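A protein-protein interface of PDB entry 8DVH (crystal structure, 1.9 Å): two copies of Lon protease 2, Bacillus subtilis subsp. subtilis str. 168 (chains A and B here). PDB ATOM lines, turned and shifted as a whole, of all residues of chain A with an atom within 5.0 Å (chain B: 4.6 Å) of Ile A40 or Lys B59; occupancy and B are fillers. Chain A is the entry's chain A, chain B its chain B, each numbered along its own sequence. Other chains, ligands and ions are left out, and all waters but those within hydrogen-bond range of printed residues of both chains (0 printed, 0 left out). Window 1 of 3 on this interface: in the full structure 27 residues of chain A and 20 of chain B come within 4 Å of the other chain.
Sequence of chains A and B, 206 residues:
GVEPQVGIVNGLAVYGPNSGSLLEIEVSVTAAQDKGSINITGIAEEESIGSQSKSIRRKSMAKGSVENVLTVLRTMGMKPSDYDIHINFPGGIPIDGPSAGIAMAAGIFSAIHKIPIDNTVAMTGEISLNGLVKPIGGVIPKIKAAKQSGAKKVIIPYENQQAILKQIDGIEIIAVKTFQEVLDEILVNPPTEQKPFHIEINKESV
O of Asn A39 is in hydrogen-bond range of N of Ile A87 (3.0 Å). The side-chain hydroxyl of Thr A41 sits at hydrogen-bond distance from a ring nitrogen (NE2) of His A86 (2.9 Å). The backbone NH of Thr A41 is in hydrogen-bond range of the backbone carbonyl oxygen of Ile A87, 2.9 Å away. O of Thr A41 sits at hydrogen-bond distance from N of Phe A89 (3.0 Å). The guanidinium group of Arg B58 lies close to the side-chain sulfur of Met B61, at 3.7 Å. OE1 of Glu B67 is in salt-bridge range of NZ of Lys B59 (2.6 Å).
Position printed for both chains: 45. Of the 10 pairs that touch across the chains among the printed residues, none has its exchanged pair printed and touching as well.
OD1 of Asn A39 lies within hydrogen-bond range of NZ of Lys B59 (2.6 Å). OE1 of Glu B67 lies within hydrogen-bond range of ND2 of Asn A39 (2.7 Å). The side-chain amino group (NZ) of Lys B59 lies within hydrogen-bond range of the backbone carbonyl oxygen (O) of Ile A40 (3.0 Å). OE1 of Glu A45 sits at hydrogen-bond distance from N of Lys B59, 2.8 Å away.
Lys B59 touches Thr A41. CG2 of Thr A41 touches OE1 of Glu B67, 3.6 Å away. C of Gly A42 touches NH1 of Arg B58 (3.8 Å). Arg B58 touches Ile A43. Glu A45 touches Arg B58. His A86 touches Glu B67 (CE1 to C, 3.7 Å).
Lys B59 touches four residues of chain A. Of the printed residues of chain B, Glu A45 touches Arg B58 and Lys B59. Of the printed residues of chain B, His A86 touches Glu B67. Printed residues of chain A within 4 Å of Arg B58: Gly A42, Ile A43 and Glu A45. Of the printed residues of chain B, Thr A41 touches Lys B59 (3.9 Å) and Glu B67 (3.6 Å). Lys B63 touches none of the printed residues of chain A. Phe A89 touches none of the printed residues of chain B. The nearest printed residue of chain A that does not touch Lys B59 is Ile A43 (5.3 Å).
Along chain B the printed residues that touch a printed residue of chain A span positions 58 to 67. Of the 11 printed residues of chain A, 7 touch a printed residue of chain B. Hydrophobic or aromatic side chains of chain A within 4 Å of the printed part of chain B: His A86. Among the printed residues, no Asp or Glu carboxylate lies within 4 Å of a Lys or Arg side-chain nitrogen of the other chain.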
ATOM      1  N   ILE A  38      14.279  16.674   6.512  1.00  0.00           N
ATOM      2  CA  ILE A  38      13.458  17.407   5.514  1.00  0.00           C
ATOM      3  C   ILE A  38      14.019  17.058   4.138  1.00  0.00           C
ATOM      4  O   ILE A  38      15.235  17.169   3.945  1.00  0.00           O
ATOM      5  CB  ILE A  38      13.422  18.925   5.800  1.00  0.00           C
ATOM      6  CG1 ILE A  38      12.513  19.663   4.813  1.00  0.00           C
ATOM      7  CG2 ILE A  38      14.811  19.551   5.821  1.00  0.00           C
ATOM      8  CD1 ILE A  38      11.091  19.247   4.824  1.00  0.00           C
ATOM      9  N   ASN A  39      13.172  16.578   3.241  1.00  0.00           N
ATOM     10  CA  ASN A  39      13.588  16.318   1.844  1.00  0.00           C
ATOM     11  C   ASN A  39      12.575  16.942   0.873  1.00  0.00           C
ATOM     12  O   ASN A  39      11.368  16.820   1.104  1.00  0.00           O
ATOM     13  CB  ASN A  39      13.768  14.830   1.637  1.00  0.00           C
ATOM     14  CG  ASN A  39      14.321  14.519   0.268  1.00  0.00           C
ATOM     15  OD1 ASN A  39      15.088  15.324  -0.278  1.00  0.00           O
ATOM     16  ND2 ASN A  39      13.935  13.363  -0.265  1.00  0.00           N
ATOM     17  N   ILE A  40      13.053  17.600  -0.171  1.00  0.00           N
ATOM     18  CA  ILE A  40      12.182  18.204  -1.197  1.00  0.00           C
ATOM     19  C   ILE A  40      12.597  17.640  -2.549  1.00  0.00           C
ATOM     20  O   ILE A  40      13.838  17.475  -2.793  1.00  0.00           O
ATOM     21  CB  ILE A  40      12.235  19.733  -1.205  1.00  0.00           C
ATOM     22  CG1 ILE A  40      12.282  20.322   0.208  1.00  0.00           C
ATOM     23  CG2 ILE A  40      11.093  20.255  -2.064  1.00  0.00           C
ATOM     24  CD1 ILE A  40      11.047  20.167   1.037  1.00  0.00           C
ATOM     25  N   THR A  41      11.611  17.256  -3.355  1.00  0.00           N
ATOM     26  CA  THR A  41      11.854  16.783  -4.730  1.00  0.00           C
ATOM     27  C   THR A  41      11.117  17.703  -5.681  1.00  0.00           C
ATOM     28  O   THR A  41      10.013  18.199  -5.331  1.00  0.00           O
ATOM     29  CB  THR A  41      11.551  15.289  -4.853  1.00  0.00           C
ATOM     30  OG1 THR A  41      10.328  14.939  -4.212  1.00  0.00           O
ATOM     31  CG2 THR A  41      12.658  14.459  -4.235  1.00  0.00           C
ATOM     32  N   GLY A  42      11.724  17.980  -6.820  1.00  0.00           N
ATOM     33  CA  GLY A  42      11.031  18.716  -7.885  1.00  0.00           C
ATOM     34  C   GLY A  42      11.451  20.177  -7.924  1.00  0.00           C
ATOM     35  O   GLY A  42      10.881  20.894  -8.780  1.00  0.00           O
ATOM     36  N   ILE A  43      12.377  20.617  -7.052  1.00  0.00           N
ATOM     37  CA  ILE A  43      12.746  22.068  -6.961  1.00  0.00           C
ATOM     38  C   ILE A  43      14.204  22.295  -7.390  1.00  0.00           C
ATOM     39  O   ILE A  43      15.046  21.386  -7.278  1.00  0.00           O
ATOM     40  CB  ILE A  43      12.482  22.690  -5.569  1.00  0.00           C
ATOM     41  CG1 ILE A  43      13.420  22.140  -4.501  1.00  0.00           C
ATOM     42  CG2 ILE A  43      11.006  22.583  -5.191  1.00  0.00           C
ATOM     43  CD1 ILE A  43      13.376  22.883  -3.205  1.00  0.00           C
ATOM     44  N   GLU A  45      17.680  23.730  -6.365  1.00  0.00           N
ATOM     45  CA  GLU A  45      18.337  23.713  -5.039  1.00  0.00           C
ATOM     46  C   GLU A  45      19.323  24.877  -4.908  1.00  0.00           C
ATOM     47  O   GLU A  45      19.473  25.325  -3.803  1.00  0.00           O
ATOM     48  CB  GLU A  45      18.975  22.356  -4.829  1.00  0.00           C
ATOM     49  CG  GLU A  45      17.875  21.315  -4.653  1.00  0.00           C
ATOM     50  CD  GLU A  45      18.483  19.993  -4.381  1.00  0.00           C
ATOM     51  OE1 GLU A  45      19.359  19.609  -5.145  1.00  0.00           O
ATOM     52  OE2 GLU A  45      18.193  19.449  -3.330  1.00  0.00           O
ATOM     53  N   VAL A  66      11.434  26.779   2.194  1.00  0.00           N
ATOM     54  CA  VAL A  66      11.358  25.585   3.089  1.00  0.00           C
ATOM     55  C   VAL A  66      11.984  25.898   4.459  1.00  0.00           C
ATOM     56  O   VAL A  66      11.392  25.527   5.492  1.00  0.00           O
ATOM     57  CB  VAL A  66      12.035  24.372   2.427  1.00  0.00           C
ATOM     58  CG1 VAL A  66      12.041  23.185   3.354  1.00  0.00           C
ATOM     59  CG2 VAL A  66      11.435  24.006   1.066  1.00  0.00           C
ATOM     60  N   HIS A  86       8.832  14.794   3.625  1.00  0.00           N
ATOM     61  CA  HIS A  86       9.161  14.762   2.185  1.00  0.00           C
ATOM     62  C   HIS A  86       8.049  15.512   1.474  1.00  0.00           C
ATOM     63  O   HIS A  86       6.856  15.110   1.584  1.00  0.00           O
ATOM     64  CB  HIS A  86       9.347  13.318   1.727  1.00  0.00           C
ATOM     65  CG  HIS A  86       9.797  13.172   0.318  1.00  0.00           C
ATOM     66  ND1 HIS A  86      10.116  11.949  -0.222  1.00  0.00           N
ATOM     67  CD2 HIS A  86       9.973  14.068  -0.674  1.00  0.00           C
ATOM     68  CE1 HIS A  86      10.479  12.102  -1.478  1.00  0.00           C
ATOM     69  NE2 HIS A  86      10.371  13.371  -1.790  1.00  0.00           N
ATOM     70  N   ILE A  87       8.437  16.536   0.747  1.00  0.00           N
ATOM     71  CA  ILE A  87       7.526  17.318  -0.114  1.00  0.00           C
ATOM     72  C   ILE A  87       7.957  17.060  -1.545  1.00  0.00           C
ATOM     73  O   ILE A  87       9.166  17.152  -1.794  1.00  0.00           O
ATOM     74  CB  ILE A  87       7.600  18.806   0.242  1.00  0.00           C
ATOM     75  CG1 ILE A  87       7.211  19.055   1.695  1.00  0.00           C
ATOM     76  CG2 ILE A  87       6.731  19.613  -0.720  1.00  0.00           C
ATOM     77  CD1 ILE A  87       7.611  20.425   2.194  1.00  0.00           C
ATOM     78  N   PHE A  89       7.064  18.101  -5.533  1.00  0.00           N
ATOM     79  CA  PHE A  89       6.504  19.009  -6.553  1.00  0.00           C
ATOM     80  C   PHE A  89       6.492  18.188  -7.838  1.00  0.00           C
ATOM     81  O   PHE A  89       7.529  17.786  -8.316  1.00  0.00           O
ATOM     82  CB  PHE A  89       7.333  20.294  -6.686  1.00  0.00           C
ATOM     83  CG  PHE A  89       7.201  21.280  -5.557  1.00  0.00           C
ATOM     84  CD1 PHE A  89       7.912  21.121  -4.378  1.00  0.00           C
ATOM     85  CD2 PHE A  89       6.355  22.366  -5.657  1.00  0.00           C
ATOM     86  CE1 PHE A  89       7.775  22.021  -3.336  1.00  0.00           C
ATOM     87  CE2 PHE A  89       6.256  23.285  -4.635  1.00  0.00           C
ATOM     88  CZ  PHE A  89       6.945  23.103  -3.464  1.00  0.00           C
ATOM     89  N   GLU B  45      23.374  12.458 -11.395  1.00  0.00           N
ATOM     90  CA  GLU B  45      23.256  12.822  -9.954  1.00  0.00           C
ATOM     91  C   GLU B  45      22.643  14.217  -9.841  1.00  0.00           C
ATOM     92  O   GLU B  45      21.929  14.453  -8.886  1.00  0.00           O
ATOM     93  CB  GLU B  45      24.595  12.842  -9.202  1.00  0.00           C
ATOM     94  CG  GLU B  45      25.318  11.500  -9.125  1.00  0.00           C
ATOM     95  CD  GLU B  45      24.981  10.579  -7.977  1.00  0.00           C
ATOM     96  OE1 GLU B  45      24.699  11.048  -6.824  1.00  0.00           O
ATOM     97  OE2 GLU B  45      24.925   9.394  -8.247  1.00  0.00           O
ATOM     98  N   GLU B  46      22.965  15.125 -10.774  1.00  0.00           N
ATOM     99  CA  GLU B  46      22.558  16.534 -10.703  1.00  0.00           C
ATOM    100  C   GLU B  46      22.259  17.011 -12.126  1.00  0.00           C
ATOM    101  O   GLU B  46      22.886  16.499 -13.057  1.00  0.00           O
ATOM    102  CB  GLU B  46      23.727  17.254 -10.041  1.00  0.00           C
ATOM    103  CG  GLU B  46      23.677  18.739  -9.977  1.00  0.00           C
ATOM    104  CD  GLU B  46      25.075  19.259  -9.621  1.00  0.00           C
ATOM    105  OE1 GLU B  46      25.504  18.939  -8.546  1.00  0.00           O
ATOM    106  OE2 GLU B  46      25.761  19.847 -10.484  1.00  0.00           O
ATOM    107  N   ARG B  58      19.971  21.227  -9.487  1.00  0.00           N
ATOM    108  CA  ARG B  58      19.185  20.391  -8.575  1.00  0.00           C
ATOM    109  C   ARG B  58      19.642  18.967  -8.664  1.00  0.00           C
ATOM    110  O   ARG B  58      20.252  18.569  -9.659  1.00  0.00           O
ATOM    111  CB  ARG B  58      17.705  20.441  -8.915  1.00  0.00           C
ATOM    112  CG  ARG B  58      17.424  20.194 -10.380  1.00  0.00           C
ATOM    113  CD  ARG B  58      15.987  19.727 -10.377  1.00  0.00           C
ATOM    114  NE  ARG B  58      15.457  19.497 -11.688  1.00  0.00           N
ATOM    115  CZ  ARG B  58      14.209  19.067 -11.908  1.00  0.00           C
ATOM    116  NH1 ARG B  58      13.409  18.804 -10.886  1.00  0.00           N
ATOM    117  NH2 ARG B  58      13.798  18.879 -13.138  1.00  0.00           N
ATOM    118  N   LYS B  59      19.334  18.221  -7.611  1.00  0.00           N
ATOM    119  CA  LYS B  59      19.515  16.769  -7.711  1.00  0.00           C
ATOM    120  C   LYS B  59      18.657  16.288  -8.869  1.00  0.00           C
ATOM    121  O   LYS B  59      17.601  16.900  -9.160  1.00  0.00           O
ATOM    122  CB  LYS B  59      19.190  16.131  -6.364  1.00  0.00           C
ATOM    123  CG  LYS B  59      17.763  16.240  -5.975  1.00  0.00           C
ATOM    124  CD  LYS B  59      17.519  15.522  -4.628  1.00  0.00           C
ATOM    125  CE  LYS B  59      16.359  16.201  -3.930  1.00  0.00           C
ATOM    126  NZ  LYS B  59      16.048  15.518  -2.650  1.00  0.00           N
ATOM    127  N   SER B  60      19.121  15.263  -9.566  1.00  0.00           N
ATOM    128  CA  SER B  60      18.487  14.776 -10.822  1.00  0.00           C
ATOM    129  C   SER B  60      17.075  14.266 -10.502  1.00  0.00           C
ATOM    130  O   SER B  60      16.837  13.840  -9.331  1.00  0.00           O
ATOM    131  CB  SER B  60      19.287  13.684 -11.487  1.00  0.00           C
ATOM    132  OG  SER B  60      19.401  12.578 -10.606  1.00  0.00           O
ATOM    133  N   MET B  61      16.204  14.328 -11.482  1.00  0.00           N
ATOM    134  CA  MET B  61      14.864  13.690 -11.463  1.00  0.00           C
ATOM    135  C   MET B  61      14.998  12.182 -11.187  1.00  0.00           C
ATOM    136  O   MET B  61      14.150  11.640 -10.461  1.00  0.00           O
ATOM    137  CB  MET B  61      14.171  13.916 -12.801  1.00  0.00           C
ATOM    138  CG  MET B  61      13.675  15.332 -12.992  1.00  0.00           C
ATOM    139  SD  MET B  61      13.072  15.563 -14.689  1.00  0.00           S
ATOM    140  CE  MET B  61      14.540  15.378 -15.684  1.00  0.00           C
ATOM    141  N   LYS B  63      17.439  10.698  -9.325  1.00  0.00           N
ATOM    142  CA  LYS B  63      17.741  10.606  -7.877  1.00  0.00           C
ATOM    143  C   LYS B  63      16.500  10.969  -7.043  1.00  0.00           C
ATOM    144  O   LYS B  63      16.216  10.251  -6.028  1.00  0.00           O
ATOM    145  CB  LYS B  63      18.946  11.497  -7.568  1.00  0.00           C
ATOM    146  CG  LYS B  63      19.396  11.421  -6.130  1.00  0.00           C
ATOM    147  CD  LYS B  63      20.078  12.703  -5.661  1.00  0.00           C
ATOM    148  CE  LYS B  63      21.026  12.460  -4.514  1.00  0.00           C
ATOM    149  NZ  LYS B  63      22.039  11.477  -4.931  1.00  0.00           N
ATOM    150  N   GLU B  67      14.060   8.725  -4.177  1.00  0.00           N
ATOM    151  CA  GLU B  67      13.630   9.208  -2.831  1.00  0.00           C
ATOM    152  C   GLU B  67      12.102   9.063  -2.698  1.00  0.00           C
ATOM    153  O   GLU B  67      11.645   8.567  -1.670  1.00  0.00           O
ATOM    154  CB  GLU B  67      14.180  10.618  -2.642  1.00  0.00           C
ATOM    155  CG  GLU B  67      15.692  10.637  -2.683  1.00  0.00           C
ATOM    156  CD  GLU B  67      16.290  12.012  -2.502  1.00  0.00           C
ATOM    157  OE1 GLU B  67      15.503  13.009  -2.472  1.00  0.00           O
ATOM    158  OE2 GLU B  67      17.551  12.094  -2.452  1.00  0.00           O
